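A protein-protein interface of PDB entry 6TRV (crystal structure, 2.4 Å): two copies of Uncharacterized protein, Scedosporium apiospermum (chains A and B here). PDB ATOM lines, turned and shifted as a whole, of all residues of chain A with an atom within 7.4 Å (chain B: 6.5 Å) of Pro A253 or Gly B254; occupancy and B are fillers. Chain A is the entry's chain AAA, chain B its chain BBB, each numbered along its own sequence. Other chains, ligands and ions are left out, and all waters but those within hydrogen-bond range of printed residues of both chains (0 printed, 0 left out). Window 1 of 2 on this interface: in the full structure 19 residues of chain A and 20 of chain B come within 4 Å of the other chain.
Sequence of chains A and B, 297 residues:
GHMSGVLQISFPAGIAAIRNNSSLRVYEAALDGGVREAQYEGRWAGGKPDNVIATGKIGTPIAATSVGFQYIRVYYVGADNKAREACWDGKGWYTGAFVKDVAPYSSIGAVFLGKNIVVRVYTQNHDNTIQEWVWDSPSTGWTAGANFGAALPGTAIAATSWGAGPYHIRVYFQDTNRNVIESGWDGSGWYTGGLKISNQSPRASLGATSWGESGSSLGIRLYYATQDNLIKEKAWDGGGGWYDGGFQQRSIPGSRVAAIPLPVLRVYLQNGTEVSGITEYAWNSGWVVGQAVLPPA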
ATOM      1  N   PHE A  11     -18.154 -24.566  18.466  1.00  0.00           N
ATOM      2  CA  PHE A  11     -19.429 -23.815  18.366  1.00  0.00           C
ATOM      3  C   PHE A  11     -19.603 -23.010  19.654  1.00  0.00           C
ATOM      4  O   PHE A  11     -19.896 -23.576  20.688  1.00  0.00           O
ATOM      5  CB  PHE A  11     -20.545 -24.854  18.167  1.00  0.00           C
ATOM      6  CG  PHE A  11     -21.938 -24.331  17.908  1.00  0.00           C
ATOM      7  CD1 PHE A  11     -22.723 -23.840  18.936  1.00  0.00           C
ATOM      8  CD2 PHE A  11     -22.475 -24.369  16.636  1.00  0.00           C
ATOM      9  CE1 PHE A  11     -24.005 -23.367  18.694  1.00  0.00           C
ATOM     10  CE2 PHE A  11     -23.768 -23.907  16.404  1.00  0.00           C
ATOM     11  CZ  PHE A  11     -24.526 -23.392  17.429  1.00  0.00           C
ATOM     12  N   PRO A  12     -19.354 -21.689  19.715  1.00  0.00           N
ATOM     13  CA  PRO A  12     -18.637 -20.952  18.675  1.00  0.00           C
ATOM     14  C   PRO A  12     -17.112 -21.110  18.745  1.00  0.00           C
ATOM     15  O   PRO A  12     -16.536 -21.291  19.809  1.00  0.00           O
ATOM     16  CB  PRO A  12     -18.949 -19.511  19.019  1.00  0.00           C
ATOM     17  CG  PRO A  12     -19.006 -19.549  20.547  1.00  0.00           C
ATOM     18  CD  PRO A  12     -19.761 -20.831  20.834  1.00  0.00           C
ATOM     19  N   ALA A  13     -16.492 -21.009  17.584  1.00  0.00           N
ATOM     20  CA  ALA A  13     -15.038 -21.086  17.394  1.00  0.00           C
ATOM     21  C   ALA A  13     -14.440 -19.685  17.478  1.00  0.00           C
ATOM     22  O   ALA A  13     -15.042 -18.753  17.042  1.00  0.00           O
ATOM     23  CB  ALA A  13     -14.766 -21.747  16.068  1.00  0.00           C
ATOM     24  N   SER A 205     -18.647 -10.127  20.277  1.00  0.00           N
ATOM     25  CA  SER A 205     -17.510 -10.430  19.382  1.00  0.00           C
ATOM     26  C   SER A 205     -17.125  -9.162  18.609  1.00  0.00           C
ATOM     27  O   SER A 205     -18.019  -8.375  18.290  1.00  0.00           O
ATOM     28  CB  SER A 205     -17.875 -11.498  18.388  1.00  0.00           C
ATOM     29  OG  SER A 205     -18.267 -12.692  18.989  1.00  0.00           O
ATOM     30  N   ASN A 229     -28.019 -11.613  17.712  1.00  0.00           N
ATOM     31  CA  ASN A 229     -27.191 -12.559  16.930  1.00  0.00           C
ATOM     32  C   ASN A 229     -27.147 -12.088  15.488  1.00  0.00           C
ATOM     33  O   ASN A 229     -27.119 -12.952  14.619  1.00  0.00           O
ATOM     34  CB  ASN A 229     -27.660 -14.007  17.029  1.00  0.00           C
ATOM     35  CG  ASN A 229     -27.735 -14.453  18.470  1.00  0.00           C
ATOM     36  OD1 ASN A 229     -26.900 -14.074  19.275  1.00  0.00           O
ATOM     37  ND2 ASN A 229     -28.809 -15.126  18.845  1.00  0.00           N
ATOM     38  N   SER A 251     -25.957 -14.805  12.749  1.00  0.00           N
ATOM     39  CA  SER A 251     -24.887 -15.700  13.249  1.00  0.00           C
ATOM     40  C   SER A 251     -25.509 -16.608  14.329  1.00  0.00           C
ATOM     41  O   SER A 251     -26.560 -16.289  14.816  1.00  0.00           O
ATOM     42  CB  SER A 251     -23.693 -14.901  13.784  1.00  0.00           C
ATOM     43  OG  SER A 251     -23.936 -14.270  15.087  1.00  0.00           O
ATOM     44  N   ILE A 252     -24.821 -17.685  14.692  1.00  0.00           N
ATOM     45  CA  ILE A 252     -25.091 -18.529  15.879  1.00  0.00           C
ATOM     46  C   ILE A 252     -24.840 -17.674  17.114  1.00  0.00           C
ATOM     47  O   ILE A 252     -24.079 -16.741  17.081  1.00  0.00           O
ATOM     48  CB  ILE A 252     -24.201 -19.788  15.865  1.00  0.00           C
ATOM     49  CG1 ILE A 252     -22.713 -19.441  15.981  1.00  0.00           C
ATOM     50  CG2 ILE A 252     -24.497 -20.722  14.678  1.00  0.00           C
ATOM     51  CD1 ILE A 252     -21.814 -20.664  16.268  1.00  0.00           C
ATOM     52  N   PRO A 253     -25.418 -17.983  18.274  1.00  0.00           N
ATOM     53  CA  PRO A 253     -25.103 -17.255  19.479  1.00  0.00           C
ATOM     54  C   PRO A 253     -23.589 -17.381  19.704  1.00  0.00           C
ATOM     55  O   PRO A 253     -23.060 -18.490  19.620  1.00  0.00           O
ATOM     56  CB  PRO A 253     -25.937 -17.907  20.616  1.00  0.00           C
ATOM     57  CG  PRO A 253     -26.993 -18.655  19.875  1.00  0.00           C
ATOM     58  CD  PRO A 253     -26.334 -19.090  18.561  1.00  0.00           C
ATOM     59  N   GLY A 254     -22.953 -16.226  19.936  1.00  0.00           N
ATOM     60  CA  GLY A 254     -21.552 -16.119  20.331  1.00  0.00           C
ATOM     61  C   GLY A 254     -20.602 -16.176  19.148  1.00  0.00           C
ATOM     62  O   GLY A 254     -19.459 -16.156  19.398  1.00  0.00           O
ATOM     63  N   SER A 255     -21.039 -16.226  17.891  1.00  0.00           N
ATOM     64  CA  SER A 255     -20.083 -16.293  16.745  1.00  0.00           C
ATOM     65  C   SER A 255     -18.978 -15.222  16.872  1.00  0.00           C
ATOM     66  O   SER A 255     -19.244 -14.075  17.172  1.00  0.00           O
ATOM     67  CB  SER A 255     -20.753 -16.156  15.426  1.00  0.00           C
ATOM     68  OG  SER A 255     -19.806 -16.310  14.362  1.00  0.00           O
ATOM     69  N   ARG A 256     -17.741 -15.633  16.733  1.00  0.00           N
ATOM     70  CA  ARG A 256     -16.619 -14.686  16.549  1.00  0.00           C
ATOM     71  C   ARG A 256     -16.769 -14.213  15.122  1.00  0.00           C
ATOM     72  O   ARG A 256     -17.559 -14.749  14.386  1.00  0.00           O
ATOM     73  CB  ARG A 256     -15.262 -15.368  16.832  1.00  0.00           C
ATOM     74  CG  ARG A 256     -14.927 -15.512  18.316  1.00  0.00           C
ATOM     75  CD  ARG A 256     -16.007 -16.263  19.097  1.00  0.00           C
ATOM     76  NE  ARG A 256     -15.538 -16.443  20.455  1.00  0.00           N
ATOM     77  CZ  ARG A 256     -16.289 -16.565  21.535  1.00  0.00           C
ATOM     78  NH1 ARG A 256     -17.601 -16.552  21.480  1.00  0.00           N
ATOM     79  NH2 ARG A 256     -15.704 -16.694  22.702  1.00  0.00           N
ATOM     80  N   GLN A 270     -19.855 -17.824  11.949  1.00  0.00           N
ATOM     81  CA  GLN A 270     -20.633 -19.082  12.023  1.00  0.00           C
ATOM     82  C   GLN A 270     -22.118 -18.681  12.037  1.00  0.00           C
ATOM     83  O   GLN A 270     -22.486 -17.936  12.944  1.00  0.00           O
ATOM     84  CB  GLN A 270     -20.266 -19.899  13.278  1.00  0.00           C
ATOM     85  CG  GLN A 270     -18.882 -20.585  13.230  1.00  0.00           C
ATOM     86  CD  GLN A 270     -18.515 -21.261  14.535  1.00  0.00           C
ATOM     87  OE1 GLN A 270     -18.506 -20.650  15.601  1.00  0.00           O
ATOM     88  NE2 GLN A 270     -18.279 -22.563  14.463  1.00  0.00           N
ATOM     89  N   PRO B  12     -20.954 -19.238  27.953  1.00  0.00           N
ATOM     90  CA  PRO B  12     -22.017 -19.592  28.903  1.00  0.00           C
ATOM     91  C   PRO B  12     -21.721 -20.876  29.710  1.00  0.00           C
ATOM     92  O   PRO B  12     -20.848 -21.638  29.312  1.00  0.00           O
ATOM     93  CB  PRO B  12     -23.164 -19.916  27.947  1.00  0.00           C
ATOM     94  CG  PRO B  12     -22.469 -20.626  26.772  1.00  0.00           C
ATOM     95  CD  PRO B  12     -21.110 -19.960  26.676  1.00  0.00           C
ATOM     96  N   ALA B  13     -22.450 -21.105  30.798  1.00  0.00           N
ATOM     97  CA  ALA B  13     -22.171 -22.187  31.778  1.00  0.00           C
ATOM     98  C   ALA B  13     -23.318 -23.226  31.692  1.00  0.00           C
ATOM     99  O   ALA B  13     -24.476 -22.762  31.518  1.00  0.00           O
ATOM    100  CB  ALA B  13     -22.025 -21.581  33.179  1.00  0.00           C
ATOM    101  N   SER B 201     -32.724 -22.740  16.478  1.00  0.00           N
ATOM    102  CA  SER B 201     -31.277 -22.435  16.324  1.00  0.00           C
ATOM    103  C   SER B 201     -30.502 -23.734  16.552  1.00  0.00           C
ATOM    104  O   SER B 201     -30.741 -24.487  17.483  1.00  0.00           O
ATOM    105  CB  SER B 201     -30.757 -21.371  17.298  1.00  0.00           C
ATOM    106  OG  SER B 201     -30.820 -20.068  16.763  1.00  0.00           O
ATOM    107  N   PRO B 202     -29.491 -24.037  15.731  1.00  0.00           N
ATOM    108  CA  PRO B 202     -28.745 -25.272  15.941  1.00  0.00           C
ATOM    109  C   PRO B 202     -28.222 -25.255  17.377  1.00  0.00           C
ATOM    110  O   PRO B 202     -27.718 -24.240  17.751  1.00  0.00           O
ATOM    111  CB  PRO B 202     -27.669 -25.233  14.864  1.00  0.00           C
ATOM    112  CG  PRO B 202     -27.662 -23.770  14.401  1.00  0.00           C
ATOM    113  CD  PRO B 202     -29.058 -23.250  14.575  1.00  0.00           C
ATOM    114  N   SER B 205     -30.340 -24.141  23.599  1.00  0.00           N
ATOM    115  CA  SER B 205     -30.482 -24.685  24.970  1.00  0.00           C
ATOM    116  C   SER B 205     -31.946 -25.104  25.281  1.00  0.00           C
ATOM    117  O   SER B 205     -32.949 -24.550  24.738  1.00  0.00           O
ATOM    118  CB  SER B 205     -29.994 -23.673  25.975  1.00  0.00           C
ATOM    119  OG  SER B 205     -28.683 -23.283  25.704  1.00  0.00           O
ATOM    120  N   ALA B 225     -34.189 -21.716  23.895  1.00  0.00           N
ATOM    121  CA  ALA B 225     -33.516 -20.528  23.325  1.00  0.00           C
ATOM    122  C   ALA B 225     -34.068 -20.224  21.931  1.00  0.00           C
ATOM    123  O   ALA B 225     -34.146 -21.168  21.115  1.00  0.00           O
ATOM    124  CB  ALA B 225     -32.020 -20.769  23.237  1.00  0.00           C
ATOM    125  N   THR B 226     -34.332 -18.953  21.649  1.00  0.00           N
ATOM    126  CA  THR B 226     -34.843 -18.465  20.358  1.00  0.00           C
ATOM    127  C   THR B 226     -33.651 -17.934  19.612  1.00  0.00           C
ATOM    128  O   THR B 226     -32.650 -17.754  20.250  1.00  0.00           O
ATOM    129  CB  THR B 226     -35.879 -17.354  20.541  1.00  0.00           C
ATOM    130  OG1 THR B 226     -35.117 -16.180  20.809  1.00  0.00           O
ATOM    131  CG2 THR B 226     -36.867 -17.634  21.647  1.00  0.00           C
ATOM    132  N   GLN B 227     -33.830 -17.604  18.344  1.00  0.00           N
ATOM    133  CA  GLN B 227     -32.734 -17.207  17.413  1.00  0.00           C
ATOM    134  C   GLN B 227     -32.114 -15.900  17.916  1.00  0.00           C
ATOM    135  O   GLN B 227     -31.027 -15.570  17.434  1.00  0.00           O
ATOM    136  CB  GLN B 227     -33.250 -17.112  15.962  1.00  0.00           C
ATOM    137  CG  GLN B 227     -34.232 -15.945  15.657  1.00  0.00           C
ATOM    138  CD  GLN B 227     -34.594 -15.734  14.187  1.00  0.00           C
ATOM    139  OE1 GLN B 227     -33.803 -15.986  13.283  1.00  0.00           O
ATOM    140  NE2 GLN B 227     -35.811 -15.291  13.907  1.00  0.00           N
ATOM    141  N   ASN B 229     -31.738 -14.657  21.293  1.00  0.00           N
ATOM    142  CA  ASN B 229     -31.171 -14.670  22.659  1.00  0.00           C
ATOM    143  C   ASN B 229     -32.277 -14.376  23.648  1.00  0.00           C
ATOM    144  O   ASN B 229     -31.975 -13.800  24.694  1.00  0.00           O
ATOM    145  CB  ASN B 229     -29.979 -13.706  22.840  1.00  0.00           C
ATOM    146  CG  ASN B 229     -28.833 -14.016  21.902  1.00  0.00           C
ATOM    147  OD1 ASN B 229     -28.502 -15.193  21.698  1.00  0.00           O
ATOM    148  ND2 ASN B 229     -28.242 -12.987  21.305  1.00  0.00           N
ATOM    149  N   SER B 251     -31.258 -13.260  27.382  1.00  0.00           N
ATOM    150  CA  SER B 251     -30.150 -14.065  27.945  1.00  0.00           C
ATOM    151  C   SER B 251     -28.861 -13.669  27.233  1.00  0.00           C
ATOM    152  O   SER B 251     -28.916 -13.030  26.180  1.00  0.00           O
ATOM    153  CB  SER B 251     -30.415 -15.527  27.800  1.00  0.00           C
ATOM    154  OG  SER B 251     -29.955 -15.978  26.539  1.00  0.00           O
ATOM    155  N   ILE B 252     -27.739 -14.037  27.807  1.00  0.00           N
ATOM    156  CA  ILE B 252     -26.460 -14.016  27.043  1.00  0.00           C
ATOM    157  C   ILE B 252     -26.564 -15.020  25.880  1.00  0.00           C
ATOM    158  O   ILE B 252     -27.338 -15.994  25.890  1.00  0.00           O
ATOM    159  CB  ILE B 252     -25.250 -14.253  27.991  1.00  0.00           C
ATOM    160  CG1 ILE B 252     -25.193 -15.677  28.525  1.00  0.00           C
ATOM    161  CG2 ILE B 252     -25.242 -13.225  29.134  1.00  0.00           C
ATOM    162  CD1 ILE B 252     -23.892 -16.044  29.139  1.00  0.00           C
ATOM    163  N   PRO B 253     -25.810 -14.786  24.789  1.00  0.00           N
ATOM    164  CA  PRO B 253     -25.683 -15.777  23.714  1.00  0.00           C
ATOM    165  C   PRO B 253     -25.270 -17.167  24.236  1.00  0.00           C
ATOM    166  O   PRO B 253     -24.267 -17.357  24.858  1.00  0.00           O
ATOM    167  CB  PRO B 253     -24.608 -15.186  22.810  1.00  0.00           C
ATOM    168  CG  PRO B 253     -24.652 -13.690  23.091  1.00  0.00           C
ATOM    169  CD  PRO B 253     -25.055 -13.552  24.546  1.00  0.00           C
ATOM    170  N   GLY B 254     -26.102 -18.162  24.005  1.00  0.00           N
ATOM    171  CA  GLY B 254     -25.821 -19.556  24.392  1.00  0.00           C
ATOM    172  C   GLY B 254     -26.127 -19.829  25.825  1.00  0.00           C
ATOM    173  O   GLY B 254     -25.827 -20.904  26.248  1.00  0.00           O
ATOM    174  N   SER B 255     -26.753 -18.915  26.547  1.00  0.00           N
ATOM    175  CA  SER B 255     -27.203 -19.237  27.918  1.00  0.00           C
ATOM    176  C   SER B 255     -27.884 -20.596  27.905  1.00  0.00           C
ATOM    177  O   SER B 255     -28.609 -20.859  26.923  1.00  0.00           O
ATOM    178  CB  SER B 255     -28.116 -18.232  28.516  1.00  0.00           C
ATOM    179  OG  SER B 255     -28.366 -18.578  29.880  1.00  0.00           O
ATOM    180  N   ARG B 256     -27.514 -21.419  28.896  1.00  0.00           N
ATOM    181  CA  ARG B 256     -28.263 -22.616  29.340  1.00  0.00           C
ATOM    182  C   ARG B 256     -29.453 -22.132  30.156  1.00  0.00           C
ATOM    183  O   ARG B 256     -29.531 -20.897  30.457  1.00  0.00           O
ATOM    184  CB  ARG B 256     -27.413 -23.580  30.178  1.00  0.00           C
ATOM    185  CG  ARG B 256     -26.460 -24.441  29.340  1.00  0.00           C
ATOM    186  CD  ARG B 256     -25.742 -23.727  28.188  1.00  0.00           C
ATOM    187  NE  ARG B 256     -24.798 -24.656  27.593  1.00  0.00           N
ATOM    188  CZ  ARG B 256     -24.186 -24.500  26.420  1.00  0.00           C
ATOM    189  NH1 ARG B 256     -24.404 -23.455  25.648  1.00  0.00           N
ATOM    190  NH2 ARG B 256     -23.422 -25.480  25.978  1.00  0.00           N
ATOM    191  N   GLN B 270     -28.433 -17.123  32.388  1.00  0.00           N
ATOM    192  CA  GLN B 270     -27.359 -16.087  32.414  1.00  0.00           C
ATOM    193  C   GLN B 270     -27.825 -14.943  31.524  1.00  0.00           C
ATOM    194  O   GLN B 270     -27.976 -15.197  30.277  1.00  0.00           O
ATOM    195  CB  GLN B 270     -26.020 -16.655  31.899  1.00  0.00           C
ATOM    196  CG  GLN B 270     -25.184 -17.363  32.959  1.00  0.00           C
ATOM    197  CD  GLN B 270     -23.898 -17.976  32.435  1.00  0.00           C
ATOM    198  OE1 GLN B 270     -23.862 -18.664  31.423  1.00  0.00           O
ATOM    199  NE2 GLN B 270     -22.798 -17.735  33.115  1.00  0.00           N
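ND2 of Asn A229 lies within hydrogen-bond range of O of Gln B227 (2.7 Å). OD1 of Asn A229 lies within hydrogen-bond range of ND2 of Asn B229, 2.7 Å away.
The backbone carbonyl oxygen (O) of Asn A229 is in hydrogen-bond range of the backbone NH (N) of Ser A251 (2.9 Å). The backbone carbonyl oxygen (O) of Gly A254 lies within hydrogen-bond range of the guanidinium group (NH1) of Arg A256, 2.8 Å away. The backbone carbonyl oxygen of Asn B229 lies within hydrogen-bond range of the backbone NH of Ser B251 (2.8 Å). The backbone carbonyl oxygen of Gly B254 lies within hydrogen-bond range of the guanidinium group of Arg B256 (3.0 Å).
Among the printed residues, pairs that only touch across the chains: Phe A11 with Pro B202, Pro A253 with Gly B254, Gly A254 with Pro B253, Pro A253 with Pro B253 and Pro A253 with Asn B229.
Pro A253 touches three residues of chain B. Of the printed residues of chain A, Asn B229 touches Asn A229 and Pro A253. Printed residues of chain A within 4 Å of Pro B253: Pro A253 (3.7 Å) and Gly A254 (3.5 Å). The nearest residue of chain A that does not touch Gly B254 is Gly A254 (5.5 Å).
Of the 12 printed residues of chain A, 4 touch a printed residue of chain B. Hydrophobic or aromatic side chains of chain A within 4 Å of the printed part of chain B: Phe A11 and Pro A253. Of the 16 printed residues of chain B, 5 touch a printed residue of chain A. Hydrophobic or aromatic side chains of chain B within 4 Å of the printed part of chain A: Pro B253. Among the printed residues, 7 pairs touch across the chains.
Asn B229 touches its own counterpart, Asn A229. Pro A253 touches Asn B229, but with the chains exchanged Asn A229 does not touch Pro B253 (4.4 Å). Pro A253 touches its own counterpart, Pro B253. Pro A253 touches Gly B254, and with the chains exchanged Gly A254 touches Pro B253. Positions printed for both chains: 12, 13, 205, 229, 251, 252, 253, 254, 255, 256 and 270.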
